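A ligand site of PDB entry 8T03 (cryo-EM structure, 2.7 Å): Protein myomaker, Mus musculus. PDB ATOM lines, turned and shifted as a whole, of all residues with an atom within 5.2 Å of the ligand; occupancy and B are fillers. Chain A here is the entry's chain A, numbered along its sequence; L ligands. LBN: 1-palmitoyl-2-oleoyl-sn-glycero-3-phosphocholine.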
ATOM      1  N   MET A  78      18.892  -9.289  20.520  1.00  0.00           N
ATOM      2  CA  MET A  78      19.856  -9.107  19.406  1.00  0.00           C
ATOM      3  C   MET A  78      19.756  -7.672  18.865  1.00  0.00           C
ATOM      4  O   MET A  78      20.813  -7.066  18.601  1.00  0.00           O
ATOM      5  CB  MET A  78      19.585 -10.096  18.266  1.00  0.00           C
ATOM      6  CG  MET A  78      19.861 -11.541  18.648  1.00  0.00           C
ATOM      7  SD  MET A  78      19.177 -12.730  17.473  1.00  0.00           S
ATOM      8  CE  MET A  78      20.030 -14.218  18.001  1.00  0.00           C
ATOM      9  N   SER A  81      21.030  -4.966  21.568  1.00  0.00           N
ATOM     10  CA  SER A  81      22.499  -5.124  21.669  1.00  0.00           C
ATOM     11  C   SER A  81      23.178  -4.321  20.561  1.00  0.00           C
ATOM     12  O   SER A  81      24.168  -3.605  20.857  1.00  0.00           O
ATOM     13  CB  SER A  81      22.936  -6.564  21.621  1.00  0.00           C
ATOM     14  OG  SER A  81      22.309  -7.323  22.651  1.00  0.00           O
ATOM     15  N   LEU A  82      22.682  -4.431  19.327  1.00  0.00           N
ATOM     16  CA  LEU A  82      23.270  -3.790  18.124  1.00  0.00           C
ATOM     17  C   LEU A  82      22.887  -2.308  18.053  1.00  0.00           C
ATOM     18  O   LEU A  82      23.703  -1.523  17.543  1.00  0.00           O
ATOM     19  CB  LEU A  82      22.826  -4.567  16.871  1.00  0.00           C
ATOM     20  CG  LEU A  82      23.395  -5.982  16.743  1.00  0.00           C
ATOM     21  CD1 LEU A  82      22.750  -6.728  15.584  1.00  0.00           C
ATOM     22  CD2 LEU A  82      24.909  -5.967  16.569  1.00  0.00           C
ATOM     23  N   TRP A 113       8.646 -19.398  13.612  1.00  0.00           N
ATOM     24  CA  TRP A 113       9.608 -20.399  13.058  1.00  0.00           C
ATOM     25  C   TRP A 113      10.000 -20.072  11.616  1.00  0.00           C
ATOM     26  O   TRP A 113      10.733 -20.891  11.025  1.00  0.00           O
ATOM     27  CB  TRP A 113       9.007 -21.816  13.139  1.00  0.00           C
ATOM     28  CG  TRP A 113       8.622 -22.232  14.521  1.00  0.00           C
ATOM     29  CD1 TRP A 113       7.368 -22.521  14.972  1.00  0.00           C
ATOM     30  CD2 TRP A 113       9.505 -22.415  15.642  1.00  0.00           C
ATOM     31  NE1 TRP A 113       7.409 -22.872  16.290  1.00  0.00           N
ATOM     32  CE2 TRP A 113       8.715 -22.812  16.731  1.00  0.00           C
ATOM     33  CE3 TRP A 113      10.892 -22.276  15.834  1.00  0.00           C
ATOM     34  CZ2 TRP A 113       9.247 -23.081  17.987  1.00  0.00           C
ATOM     35  CZ3 TRP A 113      11.428 -22.546  17.081  1.00  0.00           C
ATOM     36  CH2 TRP A 113      10.612 -22.942  18.138  1.00  0.00           C
ATOM     37  N   GLY A 114       9.544 -18.942  11.054  1.00  0.00           N
ATOM     38  CA  GLY A 114       9.804 -18.572   9.658  1.00  0.00           C
ATOM     39  C   GLY A 114      11.161 -17.899   9.484  1.00  0.00           C
ATOM     40  O   GLY A 114      11.793 -17.572  10.509  1.00  0.00           O
ATOM     41  N   TYR A 115      11.583 -17.705   8.239  1.00  0.00           N
ATOM     42  CA  TYR A 115      12.817 -16.970   7.857  1.00  0.00           C
ATOM     43  C   TYR A 115      12.656 -15.486   8.212  1.00  0.00           C
ATOM     44  O   TYR A 115      11.522 -14.963   8.102  1.00  0.00           O
ATOM     45  CB  TYR A 115      13.130 -17.136   6.364  1.00  0.00           C
ATOM     46  CG  TYR A 115      13.475 -18.550   5.959  1.00  0.00           C
ATOM     47  CD1 TYR A 115      14.684 -19.115   6.333  1.00  0.00           C
ATOM     48  CD2 TYR A 115      12.603 -19.311   5.206  1.00  0.00           C
ATOM     49  CE1 TYR A 115      15.017 -20.420   5.975  1.00  0.00           C
ATOM     50  CE2 TYR A 115      12.916 -20.612   4.840  1.00  0.00           C
ATOM     51  CZ  TYR A 115      14.127 -21.170   5.226  1.00  0.00           C
ATOM     52  OH  TYR A 115      14.443 -22.448   4.860  1.00  0.00           O
ATOM     53  N   GLY A 116      13.750 -14.834   8.623  1.00  0.00           N
ATOM     54  CA  GLY A 116      13.797 -13.397   8.931  1.00  0.00           C
ATOM     55  C   GLY A 116      13.525 -13.078  10.393  1.00  0.00           C
ATOM     56  O   GLY A 116      13.558 -11.876  10.732  1.00  0.00           O
ATOM     57  N   VAL A 117      13.260 -14.082  11.235  1.00  0.00           N
ATOM     58  CA  VAL A 117      12.872 -13.872  12.666  1.00  0.00           C
ATOM     59  C   VAL A 117      14.106 -13.417  13.477  1.00  0.00           C
ATOM     60  O   VAL A 117      13.906 -12.638  14.433  1.00  0.00           O
ATOM     61  CB  VAL A 117      12.162 -15.094  13.279  1.00  0.00           C
ATOM     62  CG1 VAL A 117      13.051 -16.337  13.366  1.00  0.00           C
ATOM     63  CG2 VAL A 117      11.563 -14.782  14.639  1.00  0.00           C
ATOM     64  N   TYR A 118      15.318 -13.869  13.124  1.00  0.00           N
ATOM     65  CA  TYR A 118      16.610 -13.414  13.722  1.00  0.00           C
ATOM     66  C   TYR A 118      17.470 -12.668  12.684  1.00  0.00           C
ATOM     67  O   TYR A 118      18.116 -11.675  13.089  1.00  0.00           O
ATOM     68  CB  TYR A 118      17.386 -14.578  14.320  1.00  0.00           C
ATOM     69  CG  TYR A 118      16.591 -15.428  15.289  1.00  0.00           C
ATOM     70  CD1 TYR A 118      16.239 -14.963  16.536  1.00  0.00           C
ATOM     71  CD2 TYR A 118      16.191 -16.706  14.940  1.00  0.00           C
ATOM     72  CE1 TYR A 118      15.510 -15.738  17.421  1.00  0.00           C
ATOM     73  CE2 TYR A 118      15.457 -17.498  15.803  1.00  0.00           C
ATOM     74  CZ  TYR A 118      15.109 -17.011  17.051  1.00  0.00           C
ATOM     75  OH  TYR A 118      14.387 -17.787  17.917  1.00  0.00           O
ATOM     76  N   SER A 119      17.489 -13.107  11.417  1.00  0.00           N
ATOM     77  CA  SER A 119      18.319 -12.504  10.339  1.00  0.00           C
ATOM     78  C   SER A 119      17.762 -11.135   9.904  1.00  0.00           C
ATOM     79  O   SER A 119      18.567 -10.321   9.411  1.00  0.00           O
ATOM     80  CB  SER A 119      18.445 -13.437   9.155  1.00  0.00           C
ATOM     81  OG  SER A 119      17.170 -13.743   8.614  1.00  0.00           O
ATOM     82  N   ILE A 122      19.196  -8.763  12.750  1.00  0.00           N
ATOM     83  CA  ILE A 122      20.687  -8.761  12.642  1.00  0.00           C
ATOM     84  C   ILE A 122      21.103  -8.071  11.330  1.00  0.00           C
ATOM     85  O   ILE A 122      22.007  -7.213  11.387  1.00  0.00           O
ATOM     86  CB  ILE A 122      21.280 -10.182  12.781  1.00  0.00           C
ATOM     87  CG1 ILE A 122      21.037 -10.764  14.178  1.00  0.00           C
ATOM     88  CG2 ILE A 122      22.755 -10.208  12.421  1.00  0.00           C
ATOM     89  CD1 ILE A 122      21.200 -12.259  14.272  1.00  0.00           C
ATOM     90  N   GLY A 123      20.448  -8.423  10.212  1.00  0.00           N
ATOM     91  CA  GLY A 123      20.714  -7.848   8.877  1.00  0.00           C
ATOM     92  C   GLY A 123      20.385  -6.366   8.805  1.00  0.00           C
ATOM     93  O   GLY A 123      21.219  -5.610   8.260  1.00  0.00           O
ATOM     94  N   THR A 126      22.780  -4.408  11.201  1.00  0.00           N
ATOM     95  CA  THR A 126      24.103  -4.389  10.537  1.00  0.00           C
ATOM     96  C   THR A 126      24.134  -3.290   9.465  1.00  0.00           C
ATOM     97  O   THR A 126      25.138  -2.539   9.423  1.00  0.00           O
ATOM     98  CB  THR A 126      24.462  -5.751   9.932  1.00  0.00           C
ATOM     99  OG1 THR A 126      24.539  -6.701  10.999  1.00  0.00           O
ATOM    100  CG2 THR A 126      25.776  -5.755   9.180  1.00  0.00           C
ATOM    101  N   GLY A 157      32.778  -9.782  19.789  1.00  0.00           N
ATOM    102  CA  GLY A 157      31.300  -9.793  19.945  1.00  0.00           C
ATOM    103  C   GLY A 157      30.609 -10.440  18.766  1.00  0.00           C
ATOM    104  O   GLY A 157      29.659 -11.226  19.001  1.00  0.00           O
ATOM    105  N   LEU A 158      31.054 -10.141  17.538  1.00  0.00           N
ATOM    106  CA  LEU A 158      30.495 -10.712  16.279  1.00  0.00           C
ATOM    107  C   LEU A 158      31.031 -12.144  16.065  1.00  0.00           C
ATOM    108  O   LEU A 158      30.327 -12.915  15.376  1.00  0.00           O
ATOM    109  CB  LEU A 158      30.829  -9.809  15.092  1.00  0.00           C
ATOM    110  CG  LEU A 158      30.170  -8.432  15.068  1.00  0.00           C
ATOM    111  CD1 LEU A 158      30.611  -7.646  13.849  1.00  0.00           C
ATOM    112  CD2 LEU A 158      28.646  -8.529  15.101  1.00  0.00           C
ATOM    113  N   GLY A 161      28.805 -14.072  18.365  1.00  0.00           N
ATOM    114  CA  GLY A 161      27.494 -13.957  17.683  1.00  0.00           C
ATOM    115  C   GLY A 161      27.362 -14.957  16.542  1.00  0.00           C
ATOM    116  O   GLY A 161      26.353 -15.690  16.529  1.00  0.00           O
ATOM    117  N   ALA A 162      28.342 -15.000  15.642  1.00  0.00           N
ATOM    118  CA  ALA A 162      28.406 -15.919  14.477  1.00  0.00           C
ATOM    119  C   ALA A 162      28.515 -17.372  14.958  1.00  0.00           C
ATOM    120  O   ALA A 162      27.892 -18.249  14.323  1.00  0.00           O
ATOM    121  CB  ALA A 162      29.570 -15.559  13.585  1.00  0.00           C
ATOM    122  N   LEU A 165      25.013 -18.420  16.305  1.00  0.00           N
ATOM    123  CA  LEU A 165      24.076 -18.617  15.162  1.00  0.00           C
ATOM    124  C   LEU A 165      24.350 -19.961  14.471  1.00  0.00           C
ATOM    125  O   LEU A 165      23.385 -20.692  14.217  1.00  0.00           O
ATOM    126  CB  LEU A 165      24.169 -17.438  14.197  1.00  0.00           C
ATOM    127  CG  LEU A 165      23.662 -16.093  14.735  1.00  0.00           C
ATOM    128  CD1 LEU A 165      24.101 -14.948  13.839  1.00  0.00           C
ATOM    129  CD2 LEU A 165      22.150 -16.093  14.899  1.00  0.00           C
ATOM    130  N   MET A 166      25.624 -20.306  14.214  1.00  0.00           N
ATOM    131  CA  MET A 166      25.984 -21.568  13.501  1.00  0.00           C
ATOM    132  C   MET A 166      25.894 -22.762  14.466  1.00  0.00           C
ATOM    133  O   MET A 166      25.716 -23.894  13.953  1.00  0.00           O
ATOM    134  CB  MET A 166      27.366 -21.506  12.847  1.00  0.00           C
ATOM    135  CG  MET A 166      28.550 -21.605  13.780  1.00  0.00           C
ATOM    136  SD  MET A 166      30.128 -21.251  12.949  1.00  0.00           S
ATOM    137  CE  MET A 166      30.135 -22.514  11.674  1.00  0.00           C
ATOM    138  N   PHE A 169      21.761 -23.017  14.273  1.00  0.00           N
ATOM    139  CA  PHE A 169      21.142 -23.151  12.928  1.00  0.00           C
ATOM    140  C   PHE A 169      21.949 -24.044  11.970  1.00  0.00           C
ATOM    141  O   PHE A 169      21.554 -24.116  10.795  1.00  0.00           O
ATOM    142  CB  PHE A 169      20.892 -21.769  12.322  1.00  0.00           C
ATOM    143  CG  PHE A 169      19.987 -20.899  13.146  1.00  0.00           C
ATOM    144  CD1 PHE A 169      18.657 -21.274  13.345  1.00  0.00           C
ATOM    145  CD2 PHE A 169      20.441 -19.732  13.742  1.00  0.00           C
ATOM    146  CE1 PHE A 169      17.814 -20.485  14.120  1.00  0.00           C
ATOM    147  CE2 PHE A 169      19.592 -18.951  14.515  1.00  0.00           C
ATOM    148  CZ  PHE A 169      18.280 -19.332  14.689  1.00  0.00           C
ATOM    149  N   PHE A 170      23.017 -24.707  12.433  1.00  0.00           N
ATOM    150  CA  PHE A 170      23.771 -25.730  11.651  1.00  0.00           C
ATOM    151  C   PHE A 170      24.102 -26.947  12.520  1.00  0.00           C
ATOM    152  O   PHE A 170      23.610 -28.043  12.197  1.00  0.00           O
ATOM    153  CB  PHE A 170      25.009 -25.115  10.984  1.00  0.00           C
ATOM    154  CG  PHE A 170      25.809 -26.099  10.164  1.00  0.00           C
ATOM    155  CD1 PHE A 170      25.322 -26.585   8.963  1.00  0.00           C
ATOM    156  CD2 PHE A 170      27.059 -26.533  10.595  1.00  0.00           C
ATOM    157  CE1 PHE A 170      26.063 -27.493   8.205  1.00  0.00           C
ATOM    158  CE2 PHE A 170      27.794 -27.435   9.834  1.00  0.00           C
ATOM    159  CZ  PHE A 170      27.297 -27.907   8.651  1.00  0.00           C
ATOM    160  N   LEU A 187      25.795 -16.702  22.886  1.00  0.00           N
ATOM    161  CA  LEU A 187      24.898 -15.536  22.627  1.00  0.00           C
ATOM    162  C   LEU A 187      24.950 -14.552  23.802  1.00  0.00           C
ATOM    163  O   LEU A 187      24.931 -13.329  23.543  1.00  0.00           O
ATOM    164  CB  LEU A 187      23.464 -16.000  22.371  1.00  0.00           C
ATOM    165  CG  LEU A 187      22.488 -14.917  21.913  1.00  0.00           C
ATOM    166  CD1 LEU A 187      22.919 -14.298  20.587  1.00  0.00           C
ATOM    167  CD2 LEU A 187      21.071 -15.453  21.804  1.00  0.00           C
ATOM    168  N   SER A 190      28.235 -12.823  23.460  1.00  0.00           N
ATOM    169  CA  SER A 190      28.087 -11.911  22.292  1.00  0.00           C
ATOM    170  C   SER A 190      27.432 -10.600  22.731  1.00  0.00           C
ATOM    171  O   SER A 190      27.952  -9.529  22.360  1.00  0.00           O
ATOM    172  CB  SER A 190      27.324 -12.557  21.161  1.00  0.00           C
ATOM    173  OG  SER A 190      27.214 -11.686  20.051  1.00  0.00           O
ATOM    174  N   PHE A 191      26.337 -10.681  23.505  1.00  0.00           N
ATOM    175  CA  PHE A 191      25.603  -9.501  24.046  1.00  0.00           C
ATOM    176  C   PHE A 191      26.520  -8.692  24.986  1.00  0.00           C
ATOM    177  O   PHE A 191      26.472  -7.453  24.897  1.00  0.00           O
ATOM    178  CB  PHE A 191      24.328  -9.922  24.791  1.00  0.00           C
ATOM    179  CG  PHE A 191      23.229 -10.560  23.981  1.00  0.00           C
ATOM    180  CD1 PHE A 191      23.147 -10.427  22.599  1.00  0.00           C
ATOM    181  CD2 PHE A 191      22.222 -11.268  24.620  1.00  0.00           C
ATOM    182  CE1 PHE A 191      22.104 -11.015  21.884  1.00  0.00           C
ATOM    183  CE2 PHE A 191      21.186 -11.863  23.908  1.00  0.00           C
ATOM    184  CZ  PHE A 191      21.131 -11.725  22.536  1.00  0.00           C
ATOM    185  N   LEU A 194      29.365  -6.973  22.626  1.00  0.00           N
ATOM    186  CA  LEU A 194      28.813  -5.955  21.677  1.00  0.00           C
ATOM    187  C   LEU A 194      28.323  -4.708  22.416  1.00  0.00           C
ATOM    188  O   LEU A 194      28.280  -3.637  21.777  1.00  0.00           O
ATOM    189  CB  LEU A 194      27.682  -6.577  20.844  1.00  0.00           C
ATOM    190  CG  LEU A 194      28.119  -7.616  19.813  1.00  0.00           C
ATOM    191  CD1 LEU A 194      26.917  -8.343  19.255  1.00  0.00           C
ATOM    192  CD2 LEU A 194      28.913  -6.986  18.678  1.00  0.00           C
HETATM  193  C1  LBN L   1      19.057 -17.618  10.849  1.00  0.00           C
HETATM  194  N1  LBN L   1      14.419 -21.437  10.531  1.00  0.00           N
HETATM  195  P1  LBN L   1      16.593 -16.812  10.238  1.00  0.00           P
HETATM  196  C2  LBN L   1      20.269 -17.561   9.938  1.00  0.00           C
HETATM  197  C3  LBN L   1      20.745 -18.923   9.507  1.00  0.00           C
HETATM  198  C4  LBN L   1      27.166 -12.045  13.344  1.00  0.00           C
HETATM  199  C5  LBN L   1      27.782  -9.625   9.673  1.00  0.00           C
HETATM  200  C6  LBN L   1      15.711 -20.664  10.384  1.00  0.00           C
HETATM  201  O1  LBN L   1      18.150 -16.533  10.491  1.00  0.00           O
HETATM  202  C7  LBN L   1      25.988 -11.413  14.038  1.00  0.00           C
HETATM  203  C8  LBN L   1      28.674  -8.709  10.451  1.00  0.00           C
HETATM  204  C9  LBN L   1      15.680 -19.214  10.811  1.00  0.00           C
HETATM  205  O2  LBN L   1      16.494 -18.390   9.947  1.00  0.00           O
HETATM  206  C10 LBN L   1      26.063 -11.481  15.534  1.00  0.00           C
HETATM  207  C11 LBN L   1      29.710  -8.019   9.599  1.00  0.00           C
HETATM  208  C12 LBN L   1      13.454 -21.025   9.471  1.00  0.00           C
HETATM  209  O3  LBN L   1      15.874 -16.499  11.531  1.00  0.00           O
HETATM  210  C13 LBN L   1      25.079 -10.594  16.254  1.00  0.00           C
HETATM  211  C14 LBN L   1      29.175  -7.417   8.313  1.00  0.00           C
HETATM  212  C15 LBN L   1      13.801 -21.207  11.875  1.00  0.00           C
HETATM  213  O4  LBN L   1      16.179 -16.113   8.975  1.00  0.00           O
HETATM  214  C16 LBN L   1      24.303 -11.297  17.333  1.00  0.00           C
HETATM  215  C18 LBN L   1      14.681 -22.893  10.385  1.00  0.00           C
HETATM  216  C19 LBN L   1      23.283 -10.438  18.019  1.00  0.00           C
HETATM  217  C21 LBN L   1      23.851  -9.556  19.103  1.00  0.00           C
HETATM  218  C25 LBN L   1      23.005 -19.622   9.396  1.00  0.00           C
HETATM  219  O5  LBN L   1      22.061 -18.807   8.924  1.00  0.00           O
HETATM  220  C26 LBN L   1      23.994 -18.894  10.258  1.00  0.00           C
HETATM  221  O6  LBN L   1      23.036 -20.793   9.155  1.00  0.00           O
HETATM  222  C27 LBN L   1      25.378 -18.862   9.670  1.00  0.00           C
HETATM  223  C28 LBN L   1      26.319 -17.907  10.402  1.00  0.00           C
HETATM  224  C29 LBN L   1      25.893 -16.456  10.379  1.00  0.00           C
HETATM  225  C30 LBN L   1      26.859 -15.513   9.709  1.00  0.00           C
HETATM  226  C31 LBN L   1      26.651 -14.068  10.101  1.00  0.00           C
HETATM  227  C32 LBN L   1      27.172 -13.731  11.458  1.00  0.00           C
HETATM  228  C33 LBN L   1      26.972 -12.297  11.874  1.00  0.00           C
HETATM  229  C34 LBN L   1      21.321 -15.523  10.710  1.00  0.00           C
HETATM  230  O7  LBN L   1      21.342 -16.868  10.651  1.00  0.00           O
HETATM  231  C35 LBN L   1      22.482 -14.879   9.992  1.00  0.00           C
HETATM  232  O8  LBN L   1      20.483 -14.910  11.320  1.00  0.00           O
HETATM  233  C36 LBN L   1      22.084 -13.914   8.921  1.00  0.00           C
HETATM  234  C37 LBN L   1      22.631 -12.510   9.151  1.00  0.00           C
HETATM  235  C38 LBN L   1      22.222 -11.495   8.107  1.00  0.00           C
HETATM  236  C39 LBN L   1      23.338 -10.590   7.622  1.00  0.00           C
HETATM  237  C40 LBN L   1      24.189  -9.949   8.723  1.00  0.00           C
HETATM  238  C41 LBN L   1      25.613 -10.418   8.750  1.00  0.00           C
HETATM  239  C42 LBN L   1      26.480  -9.590   9.649  1.00  0.00           C
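An oxygen (O4) of the ligand is in hydrogen-bond range of the side-chain hydroxyl of Ser 119 (2.6 Å).
An oxygen (O4) of the ligand lies within hydrogen-bond range of the backbone NH (N) of Gly 116, 2.8 Å away.
The backbone NH of Ser 119 sits close to an oxygen (O8) of the ligand, at 3.5 Å.
An oxygen (O3) of the ligand is in hydrogen-bond range of the backbone NH (N) of Tyr 118 (3.1 Å).
The backbone NH of Gly 161 sits close to the side-chain hydroxyl of Ser 190, at 3.3 Å.
The side-chain hydroxyl (OG1) of Thr 126 lies within hydrogen-bond range of the backbone carbonyl oxygen (O) of Ile 122, 2.6 Å away.
Residues that only touch the ligand: Trp 113 (3.1 Å), Leu 194 (3.3 Å), Val 117 (3.4 Å), Gly 161 (3.6 Å), Phe 191 (3.6 Å), Tyr 115 (3.6 Å), Met 78 (3.6 Å), Ala 162 (3.7 Å), Thr 126 (3.7 Å), Ile 122 (3.8 Å), Phe 169 (3.8 Å), Leu 158 (3.9 Å), Gly 114 (3.9 Å) and Gly 123 (3.997 Å).
Hydrophobic or aromatic side chains that line the ligand: Met 78, Tyr 115, Val 117, Tyr 118, Ile 122, Leu 158, Ala 162, Phe 169, Phe 191 and Leu 194.
Of the 25 residues printed, 17 come within 4 Å of the ligand.
Along chain A the residues within 4 Å of the ligand span positions 78 to 194.
The nearest printed residue that does not touch the ligand is Ser 190 (4.002 Å).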
